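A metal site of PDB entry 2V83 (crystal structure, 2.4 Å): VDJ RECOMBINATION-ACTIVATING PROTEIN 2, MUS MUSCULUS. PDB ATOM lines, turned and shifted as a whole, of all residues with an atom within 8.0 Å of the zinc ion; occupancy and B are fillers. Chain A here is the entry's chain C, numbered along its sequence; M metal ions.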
ATOM      1  N   TYR A  10      21.726 -22.860  -3.867  1.00  0.00           N
ATOM      2  CA  TYR A  10      20.632 -21.997  -4.276  1.00  0.00           C
ATOM      3  C   TYR A  10      19.966 -21.276  -3.115  1.00  0.00           C
ATOM      4  O   TYR A  10      19.057 -20.465  -3.323  1.00  0.00           O
ATOM      5  CB  TYR A  10      19.574 -22.841  -4.997  1.00  0.00           C
ATOM      6  CG  TYR A  10      20.066 -23.432  -6.285  1.00  0.00           C
ATOM      7  CD1 TYR A  10      20.878 -24.573  -6.297  1.00  0.00           C
ATOM      8  CD2 TYR A  10      19.792 -22.804  -7.491  1.00  0.00           C
ATOM      9  CE1 TYR A  10      21.395 -25.057  -7.486  1.00  0.00           C
ATOM     10  CE2 TYR A  10      20.302 -23.291  -8.692  1.00  0.00           C
ATOM     11  CZ  TYR A  10      21.110 -24.412  -8.682  1.00  0.00           C
ATOM     12  OH  TYR A  10      21.635 -24.869  -9.857  1.00  0.00           O
ATOM     13  N   TRP A  11      20.440 -21.541  -1.901  1.00  0.00           N
ATOM     14  CA  TRP A  11      19.823 -20.968  -0.722  1.00  0.00           C
ATOM     15  C   TRP A  11      20.498 -19.781  -0.036  1.00  0.00           C
ATOM     16  O   TRP A  11      20.167 -19.446   1.098  1.00  0.00           O
ATOM     17  CB  TRP A  11      19.582 -22.099   0.267  1.00  0.00           C
ATOM     18  CG  TRP A  11      18.963 -23.243  -0.459  1.00  0.00           C
ATOM     19  CD1 TRP A  11      19.594 -24.377  -0.901  1.00  0.00           C
ATOM     20  CD2 TRP A  11      17.617 -23.339  -0.924  1.00  0.00           C
ATOM     21  NE1 TRP A  11      18.719 -25.160  -1.612  1.00  0.00           N
ATOM     22  CE2 TRP A  11      17.498 -24.546  -1.638  1.00  0.00           C
ATOM     23  CE3 TRP A  11      16.490 -22.506  -0.800  1.00  0.00           C
ATOM     24  CZ2 TRP A  11      16.295 -24.948  -2.235  1.00  0.00           C
ATOM     25  CZ3 TRP A  11      15.301 -22.905  -1.397  1.00  0.00           C
ATOM     26  CH2 TRP A  11      15.214 -24.123  -2.108  1.00  0.00           C
ATOM     27  N   ILE A  12      21.443 -19.169  -0.731  1.00  0.00           N
ATOM     28  CA  ILE A  12      22.130 -17.998  -0.204  1.00  0.00           C
ATOM     29  C   ILE A  12      21.158 -16.823  -0.246  1.00  0.00           C
ATOM     30  O   ILE A  12      20.180 -16.840  -0.984  1.00  0.00           O
ATOM     31  CB  ILE A  12      23.337 -17.641  -1.073  1.00  0.00           C
ATOM     32  CG1 ILE A  12      22.968 -17.791  -2.553  1.00  0.00           C
ATOM     33  CG2 ILE A  12      24.525 -18.532  -0.724  1.00  0.00           C
ATOM     34  CD1 ILE A  12      23.037 -16.515  -3.354  1.00  0.00           C
ATOM     35  N   THR A  13      21.412 -15.798   0.572  1.00  0.00           N
ATOM     36  CA  THR A  13      20.582 -14.608   0.532  1.00  0.00           C
ATOM     37  C   THR A  13      21.316 -13.759  -0.501  1.00  0.00           C
ATOM     38  O   THR A  13      22.339 -13.136  -0.199  1.00  0.00           O
ATOM     39  CB  THR A  13      20.536 -13.904   1.908  1.00  0.00           C
ATOM     40  OG1 THR A  13      21.857 -13.570   2.320  1.00  0.00           O
ATOM     41  CG2 THR A  13      19.904 -14.819   2.953  1.00  0.00           C
ATOM     42  N   CYS A  14      20.810 -13.765  -1.731  1.00  0.00           N
ATOM     43  CA  CYS A  14      21.435 -13.071  -2.856  1.00  0.00           C
ATOM     44  C   CYS A  14      21.537 -11.554  -2.784  1.00  0.00           C
ATOM     45  O   CYS A  14      22.511 -10.978  -3.296  1.00  0.00           O
ATOM     46  CB  CYS A  14      20.735 -13.466  -4.166  1.00  0.00           C
ATOM     47  SG  CYS A  14      19.040 -12.834  -4.378  1.00  0.00           S
ATOM     48  N   CYS A  15      20.556 -10.896  -2.178  1.00  0.00           N
ATOM     49  CA  CYS A  15      20.556  -9.439  -2.069  1.00  0.00           C
ATOM     50  C   CYS A  15      20.007  -8.978  -0.718  1.00  0.00           C
ATOM     51  O   CYS A  15      19.489  -9.780   0.066  1.00  0.00           O
ATOM     52  CB  CYS A  15      19.743  -8.830  -3.212  1.00  0.00           C
ATOM     53  SG  CYS A  15      18.027  -9.381  -3.295  1.00  0.00           S
ATOM     54  N   PRO A  16      20.098  -7.668  -0.425  1.00  0.00           N
ATOM     55  CA  PRO A  16      19.588  -7.153   0.859  1.00  0.00           C
ATOM     56  C   PRO A  16      18.115  -7.476   1.050  1.00  0.00           C
ATOM     57  O   PRO A  16      17.643  -7.664   2.175  1.00  0.00           O
ATOM     58  CB  PRO A  16      19.825  -5.647   0.740  1.00  0.00           C
ATOM     59  CG  PRO A  16      20.951  -5.531  -0.248  1.00  0.00           C
ATOM     60  CD  PRO A  16      20.591  -6.563  -1.262  1.00  0.00           C
ATOM     61  N   THR A  17      17.403  -7.564  -0.074  1.00  0.00           N
ATOM     62  CA  THR A  17      15.981  -7.852  -0.075  1.00  0.00           C
ATOM     63  C   THR A  17      15.646  -9.336  -0.171  1.00  0.00           C
ATOM     64  O   THR A  17      14.474  -9.699  -0.081  1.00  0.00           O
ATOM     65  CB  THR A  17      15.293  -7.155  -1.265  1.00  0.00           C
ATOM     66  OG1 THR A  17      16.279  -6.809  -2.252  1.00  0.00           O
ATOM     67  CG2 THR A  17      14.576  -5.901  -0.807  1.00  0.00           C
ATOM     68  N   CYS A  18      16.673 -10.172  -0.331  1.00  0.00           N
ATOM     69  CA  CYS A  18      16.473 -11.613  -0.477  1.00  0.00           C
ATOM     70  C   CYS A  18      15.296 -12.165   0.309  1.00  0.00           C
ATOM     71  O   CYS A  18      15.265 -12.126   1.537  1.00  0.00           O
ATOM     72  CB  CYS A  18      17.743 -12.388  -0.110  1.00  0.00           C
ATOM     73  SG  CYS A  18      17.671 -14.089  -0.703  1.00  0.00           S
ATOM     74  N   ASP A  19      14.348 -12.695  -0.441  1.00  0.00           N
ATOM     75  CA  ASP A  19      13.100 -13.216   0.097  1.00  0.00           C
ATOM     76  C   ASP A  19      13.041 -14.740   0.232  1.00  0.00           C
ATOM     77  O   ASP A  19      12.119 -15.291   0.842  1.00  0.00           O
ATOM     78  CB  ASP A  19      11.963 -12.722  -0.797  1.00  0.00           C
ATOM     79  CG  ASP A  19      10.619 -12.857  -0.147  1.00  0.00           C
ATOM     80  OD1 ASP A  19      10.540 -12.639   1.079  1.00  0.00           O
ATOM     81  OD2 ASP A  19       9.640 -13.186  -0.856  1.00  0.00           O
ATOM     82  N   VAL A  20      14.035 -15.420  -0.342  1.00  0.00           N
ATOM     83  CA  VAL A  20      14.113 -16.876  -0.346  1.00  0.00           C
ATOM     84  C   VAL A  20      14.502 -17.599   0.945  1.00  0.00           C
ATOM     85  O   VAL A  20      15.600 -17.403   1.468  1.00  0.00           O
ATOM     86  CB  VAL A  20      15.067 -17.336  -1.469  1.00  0.00           C
ATOM     87  CG1 VAL A  20      15.151 -18.848  -1.503  1.00  0.00           C
ATOM     88  CG2 VAL A  20      14.589 -16.794  -2.799  1.00  0.00           C
ATOM     89  N   ASP A  21      13.593 -18.429   1.452  1.00  0.00           N
ATOM     90  CA  ASP A  21      13.822 -19.242   2.645  1.00  0.00           C
ATOM     91  C   ASP A  21      13.553 -20.689   2.242  1.00  0.00           C
ATOM     92  O   ASP A  21      12.485 -21.015   1.726  1.00  0.00           O
ATOM     93  CB  ASP A  21      12.871 -18.857   3.785  1.00  0.00           C
ATOM     94  CG  ASP A  21      13.033 -19.758   5.019  1.00  0.00           C
ATOM     95  OD1 ASP A  21      13.784 -20.760   4.939  1.00  0.00           O
ATOM     96  OD2 ASP A  21      12.411 -19.476   6.068  1.00  0.00           O
ATOM     97  N   PRO A  36      15.272 -22.539  -6.586  1.00  0.00           N
ATOM     98  CA  PRO A  36      14.920 -21.294  -7.253  1.00  0.00           C
ATOM     99  C   PRO A  36      15.745 -21.096  -8.504  1.00  0.00           C
ATOM    100  O   PRO A  36      16.779 -21.742  -8.690  1.00  0.00           O
ATOM    101  CB  PRO A  36      15.163 -20.200  -6.193  1.00  0.00           C
ATOM    102  CG  PRO A  36      16.066 -20.814  -5.211  1.00  0.00           C
ATOM    103  CD  PRO A  36      15.945 -22.314  -5.294  1.00  0.00           C
ATOM    104  N   ALA A  37      15.274 -20.214  -9.371  1.00  0.00           N
ATOM    105  CA  ALA A  37      15.957 -19.932 -10.607  1.00  0.00           C
ATOM    106  C   ALA A  37      16.941 -18.818 -10.314  1.00  0.00           C
ATOM    107  O   ALA A  37      16.615 -17.853  -9.632  1.00  0.00           O
ATOM    108  CB  ALA A  37      14.976 -19.513 -11.672  1.00  0.00           C
ATOM    109  N   MET A  38      18.166 -18.990 -10.817  1.00  0.00           N
ATOM    110  CA  MET A  38      19.192 -17.993 -10.624  1.00  0.00           C
ATOM    111  C   MET A  38      19.778 -17.540 -11.941  1.00  0.00           C
ATOM    112  O   MET A  38      19.646 -18.201 -12.978  1.00  0.00           O
ATOM    113  CB  MET A  38      20.282 -18.506  -9.701  1.00  0.00           C
ATOM    114  CG  MET A  38      19.795 -18.701  -8.272  1.00  0.00           C
ATOM    115  SD  MET A  38      21.084 -19.259  -7.156  1.00  0.00           S
ATOM    116  CE  MET A  38      21.674 -17.733  -6.476  1.00  0.00           C
ATOM    117  N   TRP A  48      25.754 -14.884  -7.962  1.00  0.00           N
ATOM    118  CA  TRP A  48      24.506 -15.442  -8.432  1.00  0.00           C
ATOM    119  C   TRP A  48      23.402 -14.787  -7.620  1.00  0.00           C
ATOM    120  O   TRP A  48      23.570 -14.510  -6.425  1.00  0.00           O
ATOM    121  CB  TRP A  48      24.460 -16.956  -8.248  1.00  0.00           C
ATOM    122  CG  TRP A  48      25.297 -17.707  -9.238  1.00  0.00           C
ATOM    123  CD1 TRP A  48      26.629 -17.949  -9.166  1.00  0.00           C
ATOM    124  CD2 TRP A  48      24.838 -18.298 -10.463  1.00  0.00           C
ATOM    125  NE1 TRP A  48      27.045 -18.660 -10.270  1.00  0.00           N
ATOM    126  CE2 TRP A  48      25.963 -18.887 -11.073  1.00  0.00           C
ATOM    127  CE3 TRP A  48      23.586 -18.387 -11.095  1.00  0.00           C
ATOM    128  CZ2 TRP A  48      25.878 -19.561 -12.304  1.00  0.00           C
ATOM    129  CZ3 TRP A  48      23.508 -19.058 -12.314  1.00  0.00           C
ATOM    130  CH2 TRP A  48      24.645 -19.637 -12.908  1.00  0.00           C
ATOM    131  N   VAL A  49      22.281 -14.498  -8.283  1.00  0.00           N
ATOM    132  CA  VAL A  49      21.154 -13.871  -7.608  1.00  0.00           C
ATOM    133  C   VAL A  49      19.877 -14.589  -8.023  1.00  0.00           C
ATOM    134  O   VAL A  49      19.788 -15.152  -9.116  1.00  0.00           O
ATOM    135  CB  VAL A  49      21.034 -12.381  -7.968  1.00  0.00           C
ATOM    136  CG1 VAL A  49      22.244 -11.628  -7.436  1.00  0.00           C
ATOM    137  CG2 VAL A  49      20.942 -12.225  -9.466  1.00  0.00           C
ATOM    138  N   HIS A  50      18.883 -14.581  -7.144  1.00  0.00           N
ATOM    139  CA  HIS A  50      17.600 -15.212  -7.421  1.00  0.00           C
ATOM    140  C   HIS A  50      16.821 -14.375  -8.425  1.00  0.00           C
ATOM    141  O   HIS A  50      16.750 -13.147  -8.304  1.00  0.00           O
ATOM    142  CB  HIS A  50      16.772 -15.367  -6.147  1.00  0.00           C
ATOM    143  CG  HIS A  50      17.433 -16.194  -5.091  1.00  0.00           C
ATOM    144  ND1 HIS A  50      17.607 -15.754  -3.800  1.00  0.00           N
ATOM    145  CD2 HIS A  50      17.944 -17.448  -5.128  1.00  0.00           C
ATOM    146  CE1 HIS A  50      18.180 -16.697  -3.078  1.00  0.00           C
ATOM    147  NE2 HIS A  50      18.387 -17.738  -3.866  1.00  0.00           N
ATOM    148  N   ALA A  51      16.226 -15.044  -9.403  1.00  0.00           N
ATOM    149  CA  ALA A  51      15.447 -14.370 -10.424  1.00  0.00           C
ATOM    150  C   ALA A  51      14.245 -13.666  -9.802  1.00  0.00           C
ATOM    151  O   ALA A  51      13.910 -12.537 -10.180  1.00  0.00           O
ATOM    152  CB  ALA A  51      14.992 -15.366 -11.454  1.00  0.00           C
ATOM    153  N   GLN A  52      13.607 -14.329  -8.841  1.00  0.00           N
ATOM    154  CA  GLN A  52      12.446 -13.774  -8.155  1.00  0.00           C
ATOM    155  C   GLN A  52      12.766 -12.497  -7.393  1.00  0.00           C
ATOM    156  O   GLN A  52      11.964 -11.559  -7.353  1.00  0.00           O
ATOM    157  CB  GLN A  52      11.882 -14.793  -7.162  1.00  0.00           C
ATOM    158  CG  GLN A  52      10.488 -15.287  -7.479  1.00  0.00           C
ATOM    159  CD  GLN A  52       9.869 -16.072  -6.334  1.00  0.00           C
ATOM    160  OE1 GLN A  52      10.504 -16.961  -5.773  1.00  0.00           O
ATOM    161  NE2 GLN A  52       8.631 -15.739  -5.995  1.00  0.00           N
ATOM    162  N   CYS A  53      13.944 -12.463  -6.783  1.00  0.00           N
ATOM    163  CA  CYS A  53      14.376 -11.296  -6.013  1.00  0.00           C
ATOM    164  C   CYS A  53      14.659 -10.096  -6.901  1.00  0.00           C
ATOM    165  O   CYS A  53      14.599  -8.956  -6.452  1.00  0.00           O
ATOM    166  CB  CYS A  53      15.597 -11.678  -5.183  1.00  0.00           C
ATOM    167  SG  CYS A  53      15.275 -13.065  -4.048  1.00  0.00           S
ATOM    168  N   MET A  54      14.965 -10.352  -8.172  1.00  0.00           N
ATOM    169  CA  MET A  54      15.219  -9.281  -9.137  1.00  0.00           C
ATOM    170  C   MET A  54      13.894  -8.921  -9.807  1.00  0.00           C
ATOM    171  O   MET A  54      13.848  -8.122 -10.733  1.00  0.00           O
ATOM    172  CB  MET A  54      16.216  -9.743 -10.209  1.00  0.00           C
ATOM    173  CG  MET A  54      17.583 -10.184  -9.689  1.00  0.00           C
ATOM    174  SD  MET A  54      18.579  -8.846  -9.007  1.00  0.00           S
ATOM    175  CE  MET A  54      18.411  -9.143  -7.303  1.00  0.00           C
HETATM  176 ZN    ZN M   1      17.223 -13.897  -3.323  1.00  0.00          ZN
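CG2 of Val 20 touches the zinc ion (3.95 Å). Five residues have an atom within 4 Å of the zinc ion: Cys 14, Cys 18, Val 20, His 50 and Cys 53.
The zinc ion is bound by ND1 of His 50 (2.0 Å), SG of Cys 53 (2.2 Å), SG of Cys 14 (2.4 Å) and SG of Cys 18 (2.7 Å). The zinc ion has four donor atoms within binding distance.
O of Tyr 10 sits at hydrogen-bond distance from NE2 of His 50 (2.9 Å). SG of Cys 53 sits close to N of Asp 19 (3.7 Å). The side-chain sulfur of Cys 14 sits close to the side-chain sulfur of Cys 15 (3.8 Å). The backbone carbonyl oxygen of Ile 12 lies close to the side-chain sulfur of Cys 18 (3.7 Å). The backbone NH (N) of Cys 18 lies within hydrogen-bond range of the side-chain sulfur (SG) of Cys 15, 3.4 Å away.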
